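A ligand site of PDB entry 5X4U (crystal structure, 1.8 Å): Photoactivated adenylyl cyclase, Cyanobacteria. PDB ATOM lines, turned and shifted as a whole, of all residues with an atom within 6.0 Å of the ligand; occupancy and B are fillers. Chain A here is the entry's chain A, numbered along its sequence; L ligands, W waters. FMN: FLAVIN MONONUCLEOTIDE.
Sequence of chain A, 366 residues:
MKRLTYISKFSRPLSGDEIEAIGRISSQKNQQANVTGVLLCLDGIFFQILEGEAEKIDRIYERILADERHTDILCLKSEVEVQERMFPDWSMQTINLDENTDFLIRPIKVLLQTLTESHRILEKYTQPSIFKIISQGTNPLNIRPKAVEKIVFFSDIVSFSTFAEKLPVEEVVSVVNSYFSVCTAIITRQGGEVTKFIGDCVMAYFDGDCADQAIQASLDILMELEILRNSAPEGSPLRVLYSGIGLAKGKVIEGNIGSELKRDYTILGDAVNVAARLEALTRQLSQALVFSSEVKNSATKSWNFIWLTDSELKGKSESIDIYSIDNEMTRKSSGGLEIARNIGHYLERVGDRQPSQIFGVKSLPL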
ATOM      1  N   TYR A   6      10.457  27.188 -15.142  1.00  0.00           N
ATOM      2  CA  TYR A   6       9.682  25.966 -14.935  1.00  0.00           C
ATOM      3  C   TYR A   6       8.407  26.300 -14.156  1.00  0.00           C
ATOM      4  O   TYR A   6       8.268  27.360 -13.535  1.00  0.00           O
ATOM      5  CB  TYR A   6      10.477  24.877 -14.179  1.00  0.00           C
ATOM      6  CG  TYR A   6      10.605  25.148 -12.693  1.00  0.00           C
ATOM      7  CD1 TYR A   6       9.604  24.754 -11.796  1.00  0.00           C
ATOM      8  CD2 TYR A   6      11.709  25.834 -12.177  1.00  0.00           C
ATOM      9  CE1 TYR A   6       9.707  25.023 -10.440  1.00  0.00           C
ATOM     10  CE2 TYR A   6      11.812  26.094 -10.827  1.00  0.00           C
ATOM     11  CZ  TYR A   6      10.819  25.692  -9.972  1.00  0.00           C
ATOM     12  OH  TYR A   6      10.913  25.963  -8.621  1.00  0.00           O
ATOM     13  N   SER A   8       5.491  24.107 -11.498  1.00  0.00           N
ATOM     14  CA  SER A   8       5.261  22.894 -10.721  1.00  0.00           C
ATOM     15  C   SER A   8       3.955  23.044  -9.969  1.00  0.00           C
ATOM     16  O   SER A   8       3.353  24.124  -9.924  1.00  0.00           O
ATOM     17  CB  SER A   8       6.414  22.640  -9.747  1.00  0.00           C
ATOM     18  OG  SER A   8       6.468  23.703  -8.803  1.00  0.00           O
ATOM     19  N   ILE A  22      10.336  28.757   2.007  1.00  0.00           N
ATOM     20  CA  ILE A  22      10.918  28.433   0.701  1.00  0.00           C
ATOM     21  C   ILE A  22      11.596  29.666   0.111  1.00  0.00           C
ATOM     22  O   ILE A  22      12.742  29.607  -0.354  1.00  0.00           O
ATOM     23  CB  ILE A  22       9.851  27.875  -0.249  1.00  0.00           C
ATOM     24  CG1 ILE A  22       9.394  26.490   0.212  1.00  0.00           C
ATOM     25  CG2 ILE A  22      10.371  27.852  -1.703  1.00  0.00           C
ATOM     26  CD1 ILE A  22       8.133  26.005  -0.444  1.00  0.00           C
ATOM     27  N   ILE A  25      14.920  30.551   2.205  1.00  0.00           N
ATOM     28  CA  ILE A  25      16.095  29.733   1.923  1.00  0.00           C
ATOM     29  C   ILE A  25      16.559  29.934   0.486  1.00  0.00           C
ATOM     30  O   ILE A  25      17.770  30.001   0.218  1.00  0.00           O
ATOM     31  CB  ILE A  25      15.828  28.247   2.210  1.00  0.00           C
ATOM     32  CG1 ILE A  25      17.055  27.402   1.839  1.00  0.00           C
ATOM     33  CG2 ILE A  25      14.632  27.740   1.421  1.00  0.00           C
ATOM     34  CD1 ILE A  25      17.151  26.095   2.587  1.00  0.00           C
ATOM     35  N   SER A  26      15.622  30.015  -0.466  1.00  0.00           N
ATOM     36  CA  SER A  26      16.009  30.153  -1.861  1.00  0.00           C
ATOM     37  C   SER A  26      16.805  31.427  -2.075  1.00  0.00           C
ATOM     38  O   SER A  26      17.848  31.425  -2.732  1.00  0.00           O
ATOM     39  CB  SER A  26      14.777  30.119  -2.768  1.00  0.00           C
ATOM     40  OG  SER A  26      14.119  28.863  -2.692  1.00  0.00           O
ATOM     41  N   SER A  27      16.325  32.539  -1.490  1.00  0.00           N
ATOM     42  CA  SER A  27      17.014  33.816  -1.656  1.00  0.00           C
ATOM     43  C   SER A  27      18.413  33.777  -1.062  1.00  0.00           C
ATOM     44  O   SER A  27      19.353  34.326  -1.641  1.00  0.00           O
ATOM     45  CB  SER A  27      16.179  34.929  -1.023  1.00  0.00           C
ATOM     46  OG  SER A  27      16.855  36.163  -1.101  1.00  0.00           O
ATOM     47  N   LYS A  29      20.355  31.033  -0.606  1.00  0.00           N
ATOM     48  CA  LYS A  29      21.209  30.170  -1.415  1.00  0.00           C
ATOM     49  C   LYS A  29      21.529  30.801  -2.770  1.00  0.00           C
ATOM     50  O   LYS A  29      22.649  30.653  -3.282  1.00  0.00           O
ATOM     51  CB  LYS A  29      20.547  28.804  -1.618  1.00  0.00           C
ATOM     52  CG  LYS A  29      20.358  28.020  -0.334  1.00  0.00           C
ATOM     53  CD  LYS A  29      21.683  27.490   0.176  1.00  0.00           C
ATOM     54  CE  LYS A  29      21.497  26.187   0.929  1.00  0.00           C
ATOM     55  NZ  LYS A  29      22.791  25.704   1.459  1.00  0.00           N
ATOM     56  N   ASN A  30      20.571  31.512  -3.355  1.00  0.00           N
ATOM     57  CA  ASN A  30      20.815  32.152  -4.650  1.00  0.00           C
ATOM     58  C   ASN A  30      21.797  33.305  -4.513  1.00  0.00           C
ATOM     59  O   ASN A  30      22.678  33.468  -5.364  1.00  0.00           O
ATOM     60  CB  ASN A  30      19.499  32.624  -5.258  1.00  0.00           C
ATOM     61  CG  ASN A  30      18.618  31.472  -5.737  1.00  0.00           C
ATOM     62  OD1 ASN A  30      19.034  30.312  -5.789  1.00  0.00           O
ATOM     63  ND2 ASN A  30      17.398  31.797  -6.104  1.00  0.00           N
ATOM     64  N   VAL A  35      22.837  33.951  -8.291  1.00  0.00           N
ATOM     65  CA  VAL A  35      21.687  33.570  -9.093  1.00  0.00           C
ATOM     66  C   VAL A  35      20.548  34.520  -8.757  1.00  0.00           C
ATOM     67  O   VAL A  35      20.326  34.845  -7.576  1.00  0.00           O
ATOM     68  CB  VAL A  35      21.308  32.098  -8.851  1.00  0.00           C
ATOM     69  CG1 VAL A  35      19.914  31.775  -9.448  1.00  0.00           C
ATOM     70  CG2 VAL A  35      22.365  31.181  -9.434  1.00  0.00           C
ATOM     71  N   LEU A  39      10.298  33.732  -8.100  1.00  0.00           N
ATOM     72  CA  LEU A  39       9.445  32.602  -7.738  1.00  0.00           C
ATOM     73  C   LEU A  39       8.044  33.141  -7.505  1.00  0.00           C
ATOM     74  O   LEU A  39       7.849  34.000  -6.635  1.00  0.00           O
ATOM     75  CB  LEU A  39       9.985  31.883  -6.505  1.00  0.00           C
ATOM     76  CG  LEU A  39       9.035  30.818  -5.966  1.00  0.00           C
ATOM     77  CD1 LEU A  39       8.791  29.722  -7.014  1.00  0.00           C
ATOM     78  CD2 LEU A  39       9.597  30.213  -4.686  1.00  0.00           C
ATOM     79  N   PHE A  46       3.499  26.650  -8.644  1.00  0.00           N
ATOM     80  CA  PHE A  46       4.720  27.440  -8.617  1.00  0.00           C
ATOM     81  C   PHE A  46       5.164  27.759 -10.036  1.00  0.00           C
ATOM     82  O   PHE A  46       5.044  26.928 -10.939  1.00  0.00           O
ATOM     83  CB  PHE A  46       5.856  26.707  -7.915  1.00  0.00           C
ATOM     84  CG  PHE A  46       5.729  26.673  -6.418  1.00  0.00           C
ATOM     85  CD1 PHE A  46       5.665  27.837  -5.677  1.00  0.00           C
ATOM     86  CD2 PHE A  46       5.711  25.452  -5.755  1.00  0.00           C
ATOM     87  CE1 PHE A  46       5.561  27.801  -4.290  1.00  0.00           C
ATOM     88  CE2 PHE A  46       5.601  25.403  -4.366  1.00  0.00           C
ATOM     89  CZ  PHE A  46       5.525  26.577  -3.641  1.00  0.00           C
ATOM     90  N   GLN A  48       8.833  29.549 -11.565  1.00  0.00           N
ATOM     91  CA  GLN A  48      10.105  30.152 -11.215  1.00  0.00           C
ATOM     92  C   GLN A  48      10.967  30.379 -12.456  1.00  0.00           C
ATOM     93  O   GLN A  48      11.034  29.522 -13.350  1.00  0.00           O
ATOM     94  CB  GLN A  48      10.883  29.308 -10.191  1.00  0.00           C
ATOM     95  CG  GLN A  48      12.106  30.030  -9.636  1.00  0.00           C
ATOM     96  CD  GLN A  48      12.841  29.266  -8.552  1.00  0.00           C
ATOM     97  OE1 GLN A  48      12.518  28.128  -8.240  1.00  0.00           O
ATOM     98  NE2 GLN A  48      13.848  29.917  -7.963  1.00  0.00           N
ATOM     99  N   LEU A  50      15.039  31.289 -13.008  1.00  0.00           N
ATOM    100  CA  LEU A  50      16.342  31.350 -12.351  1.00  0.00           C
ATOM    101  C   LEU A  50      17.413  31.593 -13.402  1.00  0.00           C
ATOM    102  O   LEU A  50      17.391  30.982 -14.469  1.00  0.00           O
ATOM    103  CB  LEU A  50      16.715  30.061 -11.625  1.00  0.00           C
ATOM    104  CG  LEU A  50      15.803  29.077 -10.911  1.00  0.00           C
ATOM    105  CD1 LEU A  50      14.942  28.276 -11.863  1.00  0.00           C
ATOM    106  CD2 LEU A  50      16.724  28.138 -10.149  1.00  0.00           C
ATOM    107  N   ILE A  60      21.403  23.956  -8.572  1.00  0.00           N
ATOM    108  CA  ILE A  60      20.199  24.450  -7.918  1.00  0.00           C
ATOM    109  C   ILE A  60      18.968  23.712  -8.447  1.00  0.00           C
ATOM    110  O   ILE A  60      18.118  23.274  -7.663  1.00  0.00           O
ATOM    111  CB  ILE A  60      20.086  25.969  -8.114  1.00  0.00           C
ATOM    112  CG1 ILE A  60      21.190  26.673  -7.323  1.00  0.00           C
ATOM    113  CG2 ILE A  60      18.695  26.469  -7.703  1.00  0.00           C
ATOM    114  CD1 ILE A  60      21.251  28.129  -7.529  1.00  0.00           C
ATOM    115  N   ARG A  63      18.501  20.255  -6.936  1.00  0.00           N
ATOM    116  CA  ARG A  63      17.848  20.230  -5.637  1.00  0.00           C
ATOM    117  C   ARG A  63      16.354  20.533  -5.745  1.00  0.00           C
ATOM    118  O   ARG A  63      15.539  19.878  -5.086  1.00  0.00           O
ATOM    119  CB  ARG A  63      18.511  21.237  -4.700  1.00  0.00           C
ATOM    120  CG  ARG A  63      20.004  21.018  -4.498  1.00  0.00           C
ATOM    121  CD  ARG A  63      20.512  21.687  -3.247  1.00  0.00           C
ATOM    122  NE  ARG A  63      20.339  23.137  -3.239  1.00  0.00           N
ATOM    123  CZ  ARG A  63      21.241  24.008  -3.713  1.00  0.00           C
ATOM    124  NH1 ARG A  63      20.987  25.312  -3.661  1.00  0.00           N
ATOM    125  NH2 ARG A  63      22.374  23.576  -4.241  1.00  0.00           N
ATOM    126  N   ILE A  64      15.988  21.520  -6.572  1.00  0.00           N
ATOM    127  CA  ILE A  64      14.580  21.834  -6.792  1.00  0.00           C
ATOM    128  C   ILE A  64      13.840  20.586  -7.284  1.00  0.00           C
ATOM    129  O   ILE A  64      12.735  20.284  -6.822  1.00  0.00           O
ATOM    130  CB  ILE A  64      14.435  23.002  -7.773  1.00  0.00           C
ATOM    131  CG1 ILE A  64      15.079  24.279  -7.236  1.00  0.00           C
ATOM    132  CG2 ILE A  64      12.972  23.261  -8.096  1.00  0.00           C
ATOM    133  CD1 ILE A  64      14.964  25.461  -8.201  1.00  0.00           C
ATOM    134  N   LEU A  65      14.447  19.835  -8.203  1.00  0.00           N
ATOM    135  CA  LEU A  65      13.792  18.639  -8.738  1.00  0.00           C
ATOM    136  C   LEU A  65      13.584  17.568  -7.675  1.00  0.00           C
ATOM    137  O   LEU A  65      12.723  16.699  -7.851  1.00  0.00           O
ATOM    138  CB  LEU A  65      14.595  18.045  -9.887  1.00  0.00           C
ATOM    139  CG  LEU A  65      14.514  18.716 -11.260  1.00  0.00           C
ATOM    140  CD1 LEU A  65      15.474  18.015 -12.195  1.00  0.00           C
ATOM    141  CD2 LEU A  65      13.091  18.652 -11.783  1.00  0.00           C
ATOM    142  N   ALA A  66      14.356  17.602  -6.590  1.00  0.00           N
ATOM    143  CA  ALA A  66      14.254  16.613  -5.523  1.00  0.00           C
ATOM    144  C   ALA A  66      13.356  17.044  -4.379  1.00  0.00           C
ATOM    145  O   ALA A  66      13.073  16.230  -3.488  1.00  0.00           O
ATOM    146  CB  ALA A  66      15.646  16.302  -4.966  1.00  0.00           C
ATOM    147  N   ASP A  67      12.890  18.294  -4.378  1.00  0.00           N
ATOM    148  CA  ASP A  67      12.124  18.830  -3.267  1.00  0.00           C
ATOM    149  C   ASP A  67      10.721  18.229  -3.281  1.00  0.00           C
ATOM    150  O   ASP A  67       9.944  18.441  -4.214  1.00  0.00           O
ATOM    151  CB  ASP A  67      12.066  20.357  -3.362  1.00  0.00           C
ATOM    152  CG  ASP A  67      11.719  21.014  -2.036  1.00  0.00           C
ATOM    153  OD1 ASP A  67      10.685  20.650  -1.436  1.00  0.00           O
ATOM    154  OD2 ASP A  67      12.474  21.909  -1.602  1.00  0.00           O
ATOM    155  N   ARG A  69       8.191  19.098  -1.706  1.00  0.00           N
ATOM    156  CA  ARG A  69       7.080  20.025  -1.503  1.00  0.00           C
ATOM    157  C   ARG A  69       6.366  20.389  -2.795  1.00  0.00           C
ATOM    158  O   ARG A  69       5.308  21.018  -2.756  1.00  0.00           O
ATOM    159  CB  ARG A  69       7.563  21.302  -0.819  1.00  0.00           C
ATOM    160  CG  ARG A  69       7.799  21.111   0.677  1.00  0.00           C
ATOM    161  CD  ARG A  69       8.617  22.242   1.264  1.00  0.00           C
ATOM    162  NE  ARG A  69       9.954  22.319   0.677  1.00  0.00           N
ATOM    163  CZ  ARG A  69      10.881  23.180   1.077  1.00  0.00           C
ATOM    164  NH1 ARG A  69      10.609  24.033   2.068  1.00  0.00           N
ATOM    165  NH2 ARG A  69      12.072  23.199   0.486  1.00  0.00           N
ATOM    166  N   HIS A  70       6.926  20.019  -3.953  1.00  0.00           N
ATOM    167  CA  HIS A  70       6.215  20.205  -5.202  1.00  0.00           C
ATOM    168  C   HIS A  70       6.472  19.003  -6.105  1.00  0.00           C
ATOM    169  O   HIS A  70       7.370  18.187  -5.865  1.00  0.00           O
ATOM    170  CB  HIS A  70       6.583  21.536  -5.902  1.00  0.00           C
ATOM    171  CG  HIS A  70       8.033  21.661  -6.278  1.00  0.00           C
ATOM    172  ND1 HIS A  70       8.488  22.674  -7.087  1.00  0.00           N
ATOM    173  CD2 HIS A  70       9.120  20.914  -5.955  1.00  0.00           C
ATOM    174  CE1 HIS A  70       9.803  22.555  -7.242  1.00  0.00           C
ATOM    175  NE2 HIS A  70      10.202  21.486  -6.568  1.00  0.00           N
ATOM    176  N   MET A  92      16.198  36.232  -5.301  1.00  0.00           N
ATOM    177  CA  MET A  92      15.002  35.402  -5.377  1.00  0.00           C
ATOM    178  C   MET A  92      13.817  36.148  -4.787  1.00  0.00           C
ATOM    179  O   MET A  92      13.349  35.822  -3.681  1.00  0.00           O
ATOM    180  CB  MET A  92      15.219  34.056  -4.677  1.00  0.00           C
ATOM    181  CG  MET A  92      14.154  32.998  -4.912  1.00  0.00           C
ATOM    182  SD  MET A  92      13.531  32.859  -6.606  1.00  0.00           S
ATOM    183  CE  MET A  92      14.993  32.874  -7.641  1.00  0.00           C
HETATM  184  N1  FMN L   1      16.591  26.427  -3.558  1.00  0.00           N
HETATM  185  C2  FMN L   1      17.563  27.248  -4.082  1.00  0.00           C
HETATM  186  O2  FMN L   1      18.720  27.193  -3.661  1.00  0.00           O
HETATM  187  N3  FMN L   1      17.256  28.132  -5.083  1.00  0.00           N
HETATM  188  C4  FMN L   1      15.967  28.205  -5.576  1.00  0.00           C
HETATM  189  O4  FMN L   1      15.707  29.010  -6.468  1.00  0.00           O
HETATM  190  C4A FMN L   1      14.981  27.382  -5.050  1.00  0.00           C
HETATM  191  N5  FMN L   1      13.686  27.442  -5.541  1.00  0.00           N
HETATM  192  C5A FMN L   1      12.715  26.621  -5.017  1.00  0.00           C
HETATM  193  C6  FMN L   1      11.423  26.682  -5.491  1.00  0.00           C
HETATM  194  C7  FMN L   1      10.437  25.851  -4.969  1.00  0.00           C
HETATM  195  C7M FMN L   1       9.049  25.941  -5.510  1.00  0.00           C
HETATM  196  C8  FMN L   1      10.742  24.938  -3.960  1.00  0.00           C
HETATM  197  C8M FMN L   1       9.682  24.046  -3.379  1.00  0.00           C
HETATM  198  C9  FMN L   1      12.042  24.883  -3.476  1.00  0.00           C
HETATM  199  C9A FMN L   1      13.033  25.719  -4.005  1.00  0.00           C
HETATM  200  N10 FMN L   1      14.333  25.655  -3.526  1.00  0.00           N
HETATM  201  C10 FMN L   1      15.305  26.484  -4.045  1.00  0.00           C
HETATM  202  C1' FMN L   1      14.680  24.713  -2.393  1.00  0.00           C
HETATM  203  C2' FMN L   1      15.501  23.509  -2.745  1.00  0.00           C
HETATM  204  O2' FMN L   1      14.616  22.554  -3.257  1.00  0.00           O
HETATM  205  C3' FMN L   1      16.151  22.936  -1.478  1.00  0.00           C
HETATM  206  O3' FMN L   1      15.212  22.840  -0.433  1.00  0.00           O
HETATM  207  C4' FMN L   1      17.329  23.752  -0.980  1.00  0.00           C
HETATM  208  O4' FMN L   1      17.840  24.605  -1.987  1.00  0.00           O
HETATM  209  C5' FMN L   1      18.400  22.746  -0.581  1.00  0.00           C
HETATM  210  O5' FMN L   1      19.149  23.227   0.504  1.00  0.00           O
HETATM  211  P   FMN L   1      20.417  22.352   0.963  1.00  0.00           P
HETATM  212  O1P FMN L   1      21.640  22.887   0.262  1.00  0.00           O
HETATM  213  O2P FMN L   1      20.586  22.440   2.462  1.00  0.00           O
HETATM  214  O3P FMN L   1      20.187  20.903   0.564  1.00  0.00           O
HETATM  215  O   HOH W   1      14.900  23.900   2.144  1.00  0.00           O
HETATM  216  O   HOH W   2      18.282  19.461  -1.984  1.00  0.00           O
HETATM  217  O   HOH W   3      23.890  22.808  -1.228  1.00  0.00           O
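OG of Ser 26 is in hydrogen-bond range of O of Ile 22, 2.8 Å away.
O of Asn 30 is in hydrogen-bond range of N of Val 35, at 3.0 Å.
A ring nitrogen (ND1) of His 70 lies within hydrogen-bond range of the side-chain hydroxyl (OG) of Ser 8 (2.8 Å).
OE1 of Gln 48 is in hydrogen-bond range of OH of Tyr 6 (2.7 Å).
OD2 of Asp 67 is in salt-bridge range of NH2 of Arg 69, 2.5 Å away.
O of Ile 64 sits at hydrogen-bond distance from NE2 of His 70, at 2.8 Å.
The side-chain sulfur (SD) of Met 92 lies close to the side-chain amide nitrogen (NE2) of Gln 48, 3.3 Å away.
The backbone NH (N) of Phe 46 sits at hydrogen-bond distance from the backbone carbonyl oxygen (O) of Ser 8 (2.8 Å).
Water W3 bridges O1P of the ligand and NH2 of Arg 63.
Water W1 lies within hydrogen-bond range of O3' of the ligand and NH2 of Arg 69.
The side-chain carboxylate (OD2) of Asp 67 lies within hydrogen-bond range of an oxygen (O2') of the ligand.
N3 of the ligand lies within hydrogen-bond range of OD1 of Asn 30, at 2.9 Å.
NE of Arg 63 is in salt-bridge range of O1P of the ligand (3.7 Å).
An oxygen (O3') of the ligand is in hydrogen-bond range of the guanidinium group (NH2) of Arg 69, 3.3 Å away.
The side-chain hydroxyl of Ser 26 lies close to a nitrogen (N5) of the ligand, 3.2 Å away.
The side-chain amino group (NZ) of Lys 29 is in salt-bridge range of an oxygen (O1P) of the ligand (3.3 Å).
NE2 of Gln 48 is in hydrogen-bond range of O4 of the ligand (2.6 Å).
An oxygen (O2') of the ligand lies within hydrogen-bond range of the backbone carbonyl oxygen of Arg 63, 3.4 Å away.
Merely in contact with the ligand: Tyr 6 (3.3 Å), Phe 46 (3.4 Å), Ile 60 (3.4 Å), Ile 64 (3.6 Å), His 70 (3.7 Å), Ile 22 (3.7 Å) and Leu 50 (3.9 Å).
Hydrophobic or aromatic side chains within 4 Å of the ligand: Ile 22, Phe 46, Leu 50, Ile 60, Ile 64 and His 70.
Within 4 Å of the ligand: Tyr 6, Ile 22, Ser 26, Lys 29, Asn 30, Phe 46, Gln 48, Leu 50, Ile 60, Arg 63, Ile 64, Asp 67, Arg 69 and His 70.
The nearest printed residue that does not touch the ligand is Leu 39 (4.1 Å).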
